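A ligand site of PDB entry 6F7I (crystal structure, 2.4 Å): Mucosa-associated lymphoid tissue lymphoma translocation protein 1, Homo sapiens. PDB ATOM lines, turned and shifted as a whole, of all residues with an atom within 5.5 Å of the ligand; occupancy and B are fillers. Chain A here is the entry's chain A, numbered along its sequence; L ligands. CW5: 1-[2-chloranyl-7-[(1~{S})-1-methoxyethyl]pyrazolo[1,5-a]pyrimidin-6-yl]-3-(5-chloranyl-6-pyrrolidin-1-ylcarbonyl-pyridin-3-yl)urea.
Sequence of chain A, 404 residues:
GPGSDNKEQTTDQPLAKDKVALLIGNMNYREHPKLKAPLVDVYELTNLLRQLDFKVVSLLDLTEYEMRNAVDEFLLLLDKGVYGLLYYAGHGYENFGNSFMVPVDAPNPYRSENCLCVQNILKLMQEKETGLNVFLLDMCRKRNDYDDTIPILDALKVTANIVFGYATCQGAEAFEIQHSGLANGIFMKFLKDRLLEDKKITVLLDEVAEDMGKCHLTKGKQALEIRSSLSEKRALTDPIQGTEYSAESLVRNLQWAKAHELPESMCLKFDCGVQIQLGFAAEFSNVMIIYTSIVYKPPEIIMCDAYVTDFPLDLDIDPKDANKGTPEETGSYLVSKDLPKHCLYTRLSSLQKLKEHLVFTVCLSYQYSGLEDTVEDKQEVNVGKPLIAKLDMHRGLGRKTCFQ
Merely in contact with the ligand: Ala 21 (3.1 Å), Gln 352 (3.2 Å), Gln 255 (3.3 Å), Lys 55 (3.3 Å), Val 57 (3.4 Å), Leu 77 (3.4 Å), Asp 392 (3.5 Å), Glu 66 (3.5 Å), Ala 70 (3.5 Å), Leu 391 (3.6 Å), Leu 22 (3.6 Å), Ile 388 (3.6 Å), Trp 256 (3.7 Å), Phe 74 (3.7 Å), Val 20 (3.7 Å), Ala 259 (3.8 Å) and Leu 59 (3.9 Å). Hydrophobic or aromatic side chains that line the ligand: Val 20, Leu 22, Val 57, Leu 59, Ala 70, Phe 74, Leu 77, Trp 256, Ala 259, Ile 388 and Leu 391. 19 residues have an atom within 4 Å of the ligand: Val 20, Ala 21, Leu 22, Lys 55, Val 57, Leu 59, Glu 66, Asn 69, Ala 70, Glu 73, Phe 74, Leu 77, Gln 255, Trp 256, Ala 259, Gln 352, Ile 388, Leu 391 and Asp 392.
ND2 of Asn 69 sits close to O of Tyr 65 (3.2 Å). NE2 of Gln 352 sits at hydrogen-bond distance from OE1 of Glu 66 (3.0 Å). N of Ile 388 lies within hydrogen-bond range of O of Ala 259 (3.4 Å). O of Val 56 lies within hydrogen-bond range of NE1 of Trp 256 (3.0 Å). The side-chain amino group (NZ) of Lys 353 is in salt-bridge range of the side-chain carboxylate (OE2) of Glu 66 (2.9 Å). The backbone carbonyl oxygen (O) of Lys 55 sits at hydrogen-bond distance from the backbone NH (N) of Ala 21 (2.9 Å). N of Val 57 sits at hydrogen-bond distance from O of Ala 21, 2.9 Å away. N of Lys 55 lies within hydrogen-bond range of O of Lys 19 (2.9 Å).
N11 of the ligand lies within hydrogen-bond range of OE1 of Glu 73 (2.8 Å). The side-chain amide nitrogen (ND2) of Asn 69 sits at hydrogen-bond distance from an oxygen (O9) of the ligand, 2.9 Å away.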
ATOM      1  N   LYS A  19     -10.503  19.079  23.512  1.00  0.00           N
ATOM      2  CA  LYS A  19      -9.197  19.650  23.759  1.00  0.00           C
ATOM      3  C   LYS A  19      -8.397  19.546  22.468  1.00  0.00           C
ATOM      4  O   LYS A  19      -8.029  18.453  22.035  1.00  0.00           O
ATOM      5  CB  LYS A  19      -8.499  18.908  24.897  1.00  0.00           C
ATOM      6  CG  LYS A  19      -9.087  19.171  26.253  1.00  0.00           C
ATOM      7  CD  LYS A  19      -8.286  18.381  27.264  1.00  0.00           C
ATOM      8  CE  LYS A  19      -8.633  18.758  28.656  1.00  0.00           C
ATOM      9  NZ  LYS A  19      -7.808  17.992  29.615  1.00  0.00           N
ATOM     10  N   VAL A  20      -8.165  20.710  21.825  1.00  0.00           N
ATOM     11  CA  VAL A  20      -7.469  20.834  20.548  1.00  0.00           C
ATOM     12  C   VAL A  20      -6.276  21.779  20.642  1.00  0.00           C
ATOM     13  O   VAL A  20      -6.345  22.765  21.362  1.00  0.00           O
ATOM     14  CB  VAL A  20      -8.432  21.188  19.374  1.00  0.00           C
ATOM     15  CG1 VAL A  20      -9.469  20.081  19.164  1.00  0.00           C
ATOM     16  CG2 VAL A  20      -9.104  22.548  19.556  1.00  0.00           C
ATOM     17  N   ALA A  21      -5.184  21.461  19.930  1.00  0.00           N
ATOM     18  CA  ALA A  21      -3.974  22.295  19.961  1.00  0.00           C
ATOM     19  C   ALA A  21      -3.238  22.375  18.625  1.00  0.00           C
ATOM     20  O   ALA A  21      -3.144  21.372  17.916  1.00  0.00           O
ATOM     21  CB  ALA A  21      -3.026  21.806  21.053  1.00  0.00           C
ATOM     22  N   LEU A  22      -2.706  23.577  18.301  1.00  0.00           N
ATOM     23  CA  LEU A  22      -1.869  23.851  17.131  1.00  0.00           C
ATOM     24  C   LEU A  22      -0.532  24.433  17.630  1.00  0.00           C
ATOM     25  O   LEU A  22      -0.498  25.466  18.286  1.00  0.00           O
ATOM     26  CB  LEU A  22      -2.534  24.788  16.113  1.00  0.00           C
ATOM     27  CG  LEU A  22      -1.654  25.247  14.925  1.00  0.00           C
ATOM     28  CD1 LEU A  22      -1.140  24.050  14.077  1.00  0.00           C
ATOM     29  CD2 LEU A  22      -2.404  26.225  14.066  1.00  0.00           C
ATOM     30  N   LYS A  55      -5.816  16.684  21.334  1.00  0.00           N
ATOM     31  CA  LYS A  55      -5.512  16.224  19.977  1.00  0.00           C
ATOM     32  C   LYS A  55      -4.553  17.361  19.520  1.00  0.00           C
ATOM     33  O   LYS A  55      -4.874  18.538  19.704  1.00  0.00           O
ATOM     34  CB  LYS A  55      -6.768  16.206  19.102  1.00  0.00           C
ATOM     35  CG  LYS A  55      -7.702  15.046  19.390  1.00  0.00           C
ATOM     36  CD  LYS A  55      -8.918  15.120  18.459  1.00  0.00           C
ATOM     37  CE  LYS A  55     -10.094  15.815  19.106  1.00  0.00           C
ATOM     38  NZ  LYS A  55     -10.591  15.044  20.272  1.00  0.00           N
ATOM     39  N   VAL A  56      -3.343  17.020  19.041  1.00  0.00           N
ATOM     40  CA  VAL A  56      -2.355  18.036  18.686  1.00  0.00           C
ATOM     41  C   VAL A  56      -1.952  18.008  17.225  1.00  0.00           C
ATOM     42  O   VAL A  56      -1.762  16.944  16.666  1.00  0.00           O
ATOM     43  CB  VAL A  56      -1.094  17.903  19.611  1.00  0.00           C
ATOM     44  CG1 VAL A  56      -0.096  19.049  19.395  1.00  0.00           C
ATOM     45  CG2 VAL A  56      -1.482  17.804  21.087  1.00  0.00           C
ATOM     46  N   VAL A  57      -1.779  19.182  16.618  1.00  0.00           N
ATOM     47  CA  VAL A  57      -1.138  19.333  15.297  1.00  0.00           C
ATOM     48  C   VAL A  57       0.174  20.079  15.591  1.00  0.00           C
ATOM     49  O   VAL A  57       0.172  21.115  16.248  1.00  0.00           O
ATOM     50  CB  VAL A  57      -2.038  19.973  14.215  1.00  0.00           C
ATOM     51  CG1 VAL A  57      -1.235  20.325  12.968  1.00  0.00           C
ATOM     52  CG2 VAL A  57      -3.153  19.005  13.839  1.00  0.00           C
ATOM     53  N   LEU A  59       3.620  21.454  13.812  1.00  0.00           N
ATOM     54  CA  LEU A  59       4.177  21.786  12.502  1.00  0.00           C
ATOM     55  C   LEU A  59       5.464  22.537  12.596  1.00  0.00           C
ATOM     56  O   LEU A  59       5.562  23.485  13.385  1.00  0.00           O
ATOM     57  CB  LEU A  59       3.133  22.559  11.638  1.00  0.00           C
ATOM     58  CG  LEU A  59       1.820  21.826  11.306  1.00  0.00           C
ATOM     59  CD1 LEU A  59       0.771  22.766  10.682  1.00  0.00           C
ATOM     60  CD2 LEU A  59       2.046  20.641  10.384  1.00  0.00           C
ATOM     61  N   LEU A  62       7.054  26.637   8.738  1.00  0.00           N
ATOM     62  CA  LEU A  62       5.960  26.963   7.814  1.00  0.00           C
ATOM     63  C   LEU A  62       6.135  28.316   7.146  1.00  0.00           C
ATOM     64  O   LEU A  62       6.570  29.277   7.782  1.00  0.00           O
ATOM     65  CB  LEU A  62       4.597  26.916   8.525  1.00  0.00           C
ATOM     66  CG  LEU A  62       4.167  25.637   9.222  1.00  0.00           C
ATOM     67  CD1 LEU A  62       2.742  25.780   9.722  1.00  0.00           C
ATOM     68  CD2 LEU A  62       4.291  24.430   8.316  1.00  0.00           C
ATOM     69  N   TYR A  65       1.686  31.421   3.800  1.00  0.00           N
ATOM     70  CA  TYR A  65       0.458  30.750   3.326  1.00  0.00           C
ATOM     71  C   TYR A  65       0.123  29.506   4.181  1.00  0.00           C
ATOM     72  O   TYR A  65      -1.030  29.318   4.556  1.00  0.00           O
ATOM     73  CB  TYR A  65       0.577  30.444   1.816  1.00  0.00           C
ATOM     74  CG  TYR A  65      -0.450  29.490   1.235  1.00  0.00           C
ATOM     75  CD1 TYR A  65      -1.745  29.917   0.933  1.00  0.00           C
ATOM     76  CD2 TYR A  65      -0.102  28.177   0.887  1.00  0.00           C
ATOM     77  CE1 TYR A  65      -2.688  29.051   0.360  1.00  0.00           C
ATOM     78  CE2 TYR A  65      -1.031  27.308   0.315  1.00  0.00           C
ATOM     79  CZ  TYR A  65      -2.321  27.745   0.058  1.00  0.00           C
ATOM     80  OH  TYR A  65      -3.245  26.899  -0.508  1.00  0.00           O
ATOM     81  N   GLU A  66       1.151  28.719   4.543  1.00  0.00           N
ATOM     82  CA  GLU A  66       1.029  27.513   5.384  1.00  0.00           C
ATOM     83  C   GLU A  66       0.563  27.848   6.785  1.00  0.00           C
ATOM     84  O   GLU A  66      -0.400  27.227   7.274  1.00  0.00           O
ATOM     85  CB  GLU A  66       2.341  26.712   5.383  1.00  0.00           C
ATOM     86  CG  GLU A  66       2.624  25.982   4.063  1.00  0.00           C
ATOM     87  CD  GLU A  66       4.086  25.587   3.816  1.00  0.00           C
ATOM     88  OE1 GLU A  66       4.924  25.766   4.728  1.00  0.00           O
ATOM     89  OE2 GLU A  66       4.385  25.081   2.711  1.00  0.00           O
ATOM     90  N   ASN A  69      -3.175  29.037   6.740  1.00  0.00           N
ATOM     91  CA  ASN A  69      -4.072  27.889   6.564  1.00  0.00           C
ATOM     92  C   ASN A  69      -4.220  27.132   7.854  1.00  0.00           C
ATOM     93  O   ASN A  69      -5.364  26.794   8.238  1.00  0.00           O
ATOM     94  CB  ASN A  69      -3.511  26.911   5.509  1.00  0.00           C
ATOM     95  CG  ASN A  69      -3.533  27.416   4.108  1.00  0.00           C
ATOM     96  OD1 ASN A  69      -4.319  28.309   3.750  1.00  0.00           O
ATOM     97  ND2 ASN A  69      -2.665  26.836   3.288  1.00  0.00           N
ATOM     98  N   ALA A  70      -3.069  26.873   8.556  1.00  0.00           N
ATOM     99  CA  ALA A  70      -3.040  26.150   9.825  1.00  0.00           C
ATOM    100  C   ALA A  70      -3.839  26.889  10.912  1.00  0.00           C
ATOM    101  O   ALA A  70      -4.718  26.267  11.526  1.00  0.00           O
ATOM    102  CB  ALA A  70      -1.598  25.880  10.254  1.00  0.00           C
ATOM    103  N   GLU A  73      -7.723  27.117  10.188  1.00  0.00           N
ATOM    104  CA  GLU A  73      -8.364  25.812  10.413  1.00  0.00           C
ATOM    105  C   GLU A  73      -8.427  25.446  11.887  1.00  0.00           C
ATOM    106  O   GLU A  73      -9.379  24.780  12.307  1.00  0.00           O
ATOM    107  CB  GLU A  73      -7.671  24.721   9.614  1.00  0.00           C
ATOM    108  CG  GLU A  73      -8.045  24.730   8.147  1.00  0.00           C
ATOM    109  CD  GLU A  73      -7.471  23.587   7.326  1.00  0.00           C
ATOM    110  OE1 GLU A  73      -7.056  22.552   7.898  1.00  0.00           O
ATOM    111  OE2 GLU A  73      -7.432  23.743   6.088  1.00  0.00           O
ATOM    112  N   PHE A  74      -7.441  25.885  12.692  1.00  0.00           N
ATOM    113  CA  PHE A  74      -7.444  25.645  14.131  1.00  0.00           C
ATOM    114  C   PHE A  74      -8.644  26.392  14.775  1.00  0.00           C
ATOM    115  O   PHE A  74      -9.342  25.835  15.633  1.00  0.00           O
ATOM    116  CB  PHE A  74      -6.130  26.114  14.757  1.00  0.00           C
ATOM    117  CG  PHE A  74      -6.152  26.259  16.250  1.00  0.00           C
ATOM    118  CD1 PHE A  74      -6.106  25.150  17.082  1.00  0.00           C
ATOM    119  CD2 PHE A  74      -6.208  27.515  16.842  1.00  0.00           C
ATOM    120  CE1 PHE A  74      -6.123  25.278  18.471  1.00  0.00           C
ATOM    121  CE2 PHE A  74      -6.247  27.642  18.233  1.00  0.00           C
ATOM    122  CZ  PHE A  74      -6.186  26.521  19.034  1.00  0.00           C
ATOM    123  N   LEU A  77     -12.203  24.944  14.735  1.00  0.00           N
ATOM    124  CA  LEU A  77     -12.394  23.867  15.696  1.00  0.00           C
ATOM    125  C   LEU A  77     -12.891  24.393  17.029  1.00  0.00           C
ATOM    126  O   LEU A  77     -13.291  23.605  17.882  1.00  0.00           O
ATOM    127  CB  LEU A  77     -11.044  23.158  15.984  1.00  0.00           C
ATOM    128  CG  LEU A  77     -10.269  22.462  14.862  1.00  0.00           C
ATOM    129  CD1 LEU A  77      -8.960  22.017  15.376  1.00  0.00           C
ATOM    130  CD2 LEU A  77     -11.002  21.276  14.318  1.00  0.00           C
ATOM    131  N   ARG A 252     -14.186  17.550  14.295  1.00  0.00           N
ATOM    132  CA  ARG A 252     -12.914  17.790  14.977  1.00  0.00           C
ATOM    133  C   ARG A 252     -12.021  16.581  14.974  1.00  0.00           C
ATOM    134  O   ARG A 252     -10.836  16.694  14.623  1.00  0.00           O
ATOM    135  CB  ARG A 252     -13.106  18.357  16.416  1.00  0.00           C
ATOM    136  CG  ARG A 252     -13.812  19.705  16.464  1.00  0.00           C
ATOM    137  CD  ARG A 252     -13.911  20.318  17.867  1.00  0.00           C
ATOM    138  NE  ARG A 252     -14.504  19.403  18.850  1.00  0.00           N
ATOM    139  CZ  ARG A 252     -15.769  19.447  19.272  1.00  0.00           C
ATOM    140  NH1 ARG A 252     -16.197  18.587  20.177  1.00  0.00           N
ATOM    141  NH2 ARG A 252     -16.618  20.316  18.757  1.00  0.00           N
ATOM    142  N   GLN A 255     -10.918  15.584  11.178  1.00  0.00           N
ATOM    143  CA  GLN A 255      -9.903  16.494  10.660  1.00  0.00           C
ATOM    144  C   GLN A 255      -8.520  16.225  11.266  1.00  0.00           C
ATOM    145  O   GLN A 255      -7.526  16.178  10.542  1.00  0.00           O
ATOM    146  CB  GLN A 255     -10.363  17.945  10.820  1.00  0.00           C
ATOM    147  CG  GLN A 255     -11.381  18.386   9.736  1.00  0.00           C
ATOM    148  CD  GLN A 255     -10.818  18.277   8.315  1.00  0.00           C
ATOM    149  OE1 GLN A 255     -11.013  17.282   7.604  1.00  0.00           O
ATOM    150  NE2 GLN A 255     -10.077  19.272   7.898  1.00  0.00           N
ATOM    151  N   TRP A 256      -8.481  15.912  12.552  1.00  0.00           N
ATOM    152  CA  TRP A 256      -7.220  15.596  13.184  1.00  0.00           C
ATOM    153  C   TRP A 256      -6.713  14.195  12.791  1.00  0.00           C
ATOM    154  O   TRP A 256      -5.514  14.037  12.578  1.00  0.00           O
ATOM    155  CB  TRP A 256      -7.332  15.806  14.697  1.00  0.00           C
ATOM    156  CG  TRP A 256      -6.167  15.275  15.459  1.00  0.00           C
ATOM    157  CD1 TRP A 256      -4.967  15.872  15.655  1.00  0.00           C
ATOM    158  CD2 TRP A 256      -6.074  13.976  16.040  1.00  0.00           C
ATOM    159  NE1 TRP A 256      -4.117  15.036  16.328  1.00  0.00           N
ATOM    160  CE2 TRP A 256      -4.774  13.863  16.586  1.00  0.00           C
ATOM    161  CE3 TRP A 256      -6.968  12.892  16.153  1.00  0.00           C
ATOM    162  CZ2 TRP A 256      -4.346  12.703  17.252  1.00  0.00           C
ATOM    163  CZ3 TRP A 256      -6.550  11.744  16.808  1.00  0.00           C
ATOM    164  CH2 TRP A 256      -5.252  11.655  17.348  1.00  0.00           C
ATOM    165  N   ALA A 259      -5.097  13.930   9.238  1.00  0.00           N
ATOM    166  CA  ALA A 259      -3.758  14.500   9.125  1.00  0.00           C
ATOM    167  C   ALA A 259      -2.683  13.681   9.839  1.00  0.00           C
ATOM    168  O   ALA A 259      -1.530  14.085   9.836  1.00  0.00           O
ATOM    169  CB  ALA A 259      -3.779  15.921   9.663  1.00  0.00           C
ATOM    170  N   GLN A 352       4.076  19.126   3.985  1.00  0.00           N
ATOM    171  CA  GLN A 352       3.040  20.022   3.425  1.00  0.00           C
ATOM    172  C   GLN A 352       3.388  20.546   1.997  1.00  0.00           C
ATOM    173  O   GLN A 352       2.525  21.054   1.303  1.00  0.00           O
ATOM    174  CB  GLN A 352       2.748  21.191   4.394  1.00  0.00           C
ATOM    175  CG  GLN A 352       3.808  22.292   4.421  1.00  0.00           C
ATOM    176  CD  GLN A 352       5.073  22.020   5.202  1.00  0.00           C
ATOM    177  OE1 GLN A 352       5.308  20.936   5.702  1.00  0.00           O
ATOM    178  NE2 GLN A 352       5.924  23.021   5.350  1.00  0.00           N
ATOM    179  N   LYS A 353       4.651  20.388   1.566  1.00  0.00           N
ATOM    180  CA  LYS A 353       5.132  20.795   0.238  1.00  0.00           C
ATOM    181  C   LYS A 353       4.872  19.727  -0.827  1.00  0.00           C
ATOM    182  O   LYS A 353       5.026  19.998  -2.017  1.00  0.00           O
ATOM    183  CB  LYS A 353       6.606  21.203   0.318  1.00  0.00           C
ATOM    184  CG  LYS A 353       6.738  22.569   0.954  1.00  0.00           C
ATOM    185  CD  LYS A 353       8.152  22.967   1.274  1.00  0.00           C
ATOM    186  CE  LYS A 353       8.187  23.975   2.414  1.00  0.00           C
ATOM    187  NZ  LYS A 353       7.258  25.138   2.222  1.00  0.00           N
ATOM    188  N   LEU A 354       4.409  18.541  -0.419  1.00  0.00           N
ATOM    189  CA  LEU A 354       4.071  17.427  -1.291  1.00  0.00           C
ATOM    190  C   LEU A 354       2.729  17.713  -1.996  1.00  0.00           C
ATOM    191  O   LEU A 354       1.684  17.787  -1.356  1.00  0.00           O
ATOM    192  CB  LEU A 354       4.009  16.129  -0.457  1.00  0.00           C
ATOM    193  CG  LEU A 354       4.052  14.799  -1.169  1.00  0.00           C
ATOM    194  CD1 LEU A 354       5.469  14.463  -1.660  1.00  0.00           C
ATOM    195  CD2 LEU A 354       3.521  13.707  -0.265  1.00  0.00           C
ATOM    196  N   ILE A 388       0.211  15.497   7.287  1.00  0.00           N
ATOM    197  CA  ILE A 388      -0.434  16.761   6.860  1.00  0.00           C
ATOM    198  C   ILE A 388      -0.581  16.913   5.326  1.00  0.00           C
ATOM    199  O   ILE A 388      -1.376  17.758   4.878  1.00  0.00           O
ATOM    200  CB  ILE A 388       0.272  18.000   7.519  1.00  0.00           C
ATOM    201  CG1 ILE A 388      -0.705  19.206   7.719  1.00  0.00           C
ATOM    202  CG2 ILE A 388       1.524  18.416   6.780  1.00  0.00           C
ATOM    203  CD1 ILE A 388      -1.634  19.142   8.983  1.00  0.00           C
ATOM    204  N   ALA A 389       0.178  16.117   4.531  1.00  0.00           N
ATOM    205  CA  ALA A 389       0.109  16.149   3.053  1.00  0.00           C
ATOM    206  C   ALA A 389      -1.264  15.657   2.533  1.00  0.00           C
ATOM    207  O   ALA A 389      -1.660  16.047   1.442  1.00  0.00           O
ATOM    208  CB  ALA A 389       1.238  15.326   2.442  1.00  0.00           C
ATOM    209  N   LEU A 391      -4.085  16.671   3.498  1.00  0.00           N
ATOM    210  CA  LEU A 391      -4.982  17.827   3.494  1.00  0.00           C
ATOM    211  C   LEU A 391      -5.107  18.496   2.122  1.00  0.00           C
ATOM    212  O   LEU A 391      -6.243  18.640   1.677  1.00  0.00           O
ATOM    213  CB  LEU A 391      -4.631  18.835   4.602  1.00  0.00           C
ATOM    214  CG  LEU A 391      -5.389  18.655   5.947  1.00  0.00           C
ATOM    215  CD1 LEU A 391      -5.378  17.196   6.463  1.00  0.00           C
ATOM    216  CD2 LEU A 391      -4.833  19.553   7.011  1.00  0.00           C
ATOM    217  N   ASP A 392      -3.985  18.839   1.420  1.00  0.00           N
ATOM    218  CA  ASP A 392      -4.009  19.489   0.093  1.00  0.00           C
ATOM    219  C   ASP A 392      -4.692  20.865   0.116  1.00  0.00           C
ATOM    220  O   ASP A 392      -4.861  21.506  -0.923  1.00  0.00           O
ATOM    221  CB  ASP A 392      -4.631  18.581  -0.994  1.00  0.00           C
ATOM    222  CG  ASP A 392      -3.874  17.306  -1.270  1.00  0.00           C
ATOM    223  OD1 ASP A 392      -2.652  17.387  -1.545  1.00  0.00           O
ATOM    224  OD2 ASP A 392      -4.503  16.219  -1.275  1.00  0.00           O
HETATM  225  C1  CW5 L   1      -3.398  22.978   7.525  1.00  0.00           C
HETATM  226  C2  CW5 L   1      -1.993  23.026   7.710  1.00  0.00           C
HETATM  227  C3  CW5 L   1      -1.180  23.281   6.598  1.00  0.00           C
HETATM  228  C12 CW5 L   1      -5.425  22.059  11.876  1.00  0.00           C
HETATM  229  C13 CW5 L   1      -6.040  20.948  12.382  1.00  0.00           C
HETATM  230  C15 CW5 L   1      -4.724  22.999  12.808  1.00  0.00           C
HETATM  231  C16 CW5 L   1      -5.413  21.565  14.527  1.00  0.00           C
HETATM  232  C19 CW5 L   1      -6.208  19.908  15.666  1.00  0.00           C
HETATM  233  C20 CW5 L   1      -5.464  21.171  15.799  1.00  0.00           C
HETATM  234  C22 CW5 L   1      -6.798  19.865  11.553  1.00  0.00           C
HETATM  235  C24 CW5 L   1      -5.804  18.970  10.739  1.00  0.00           C
HETATM  236  C26 CW5 L   1      -4.186  22.505   9.828  1.00  0.00           C
HETATM  237  C28 CW5 L   1      -8.816  21.219  11.083  1.00  0.00           C
HETATM  238  C29 CW5 L   1      -0.178  22.638   1.977  1.00  0.00           C
HETATM  239  C30 CW5 L   1      -0.879  21.457   1.253  1.00  0.00           C
HETATM  240  C4  CW5 L   1      -1.776  23.488   5.342  1.00  0.00           C
HETATM  241  N5  CW5 L   1      -3.115  23.401   5.210  1.00  0.00           N
HETATM  242  C6  CW5 L   1      -3.943  23.147   6.243  1.00  0.00           C
HETATM  243 CL7  CW5 L   1       0.556  23.333   6.759  1.00  0.00          CL
HETATM  244  C8  CW5 L   1      -1.018  23.627   4.058  1.00  0.00           C
HETATM  245  O9  CW5 L   1      -0.633  24.756   3.734  1.00  0.00           O
HETATM  246  N10 CW5 L   1      -0.836  22.531   3.276  1.00  0.00           N
HETATM  247  N11 CW5 L   1      -4.365  22.772   8.530  1.00  0.00           N
HETATM  248  N14 CW5 L   1      -4.727  22.740  14.052  1.00  0.00           N
HETATM  249  N17 CW5 L   1      -6.028  20.758  13.697  1.00  0.00           N
HETATM  250  N18 CW5 L   1      -6.525  19.756  14.452  1.00  0.00           N
HETATM  251 CL2  CW5 L   1      -6.693  18.885  16.956  1.00  0.00          CL
HETATM  252  O23 CW5 L   1      -7.720  20.419  10.574  1.00  0.00           O
HETATM  253  N25 CW5 L   1      -5.324  22.292  10.539  1.00  0.00           N
HETATM  254  O27 CW5 L   1      -3.061  22.500  10.326  1.00  0.00           O
HETATM  255  C31 CW5 L   1      -0.991  20.362   2.341  1.00  0.00           C
HETATM  256  C32 CW5 L   1      -1.316  21.183   3.627  1.00  0.00           C
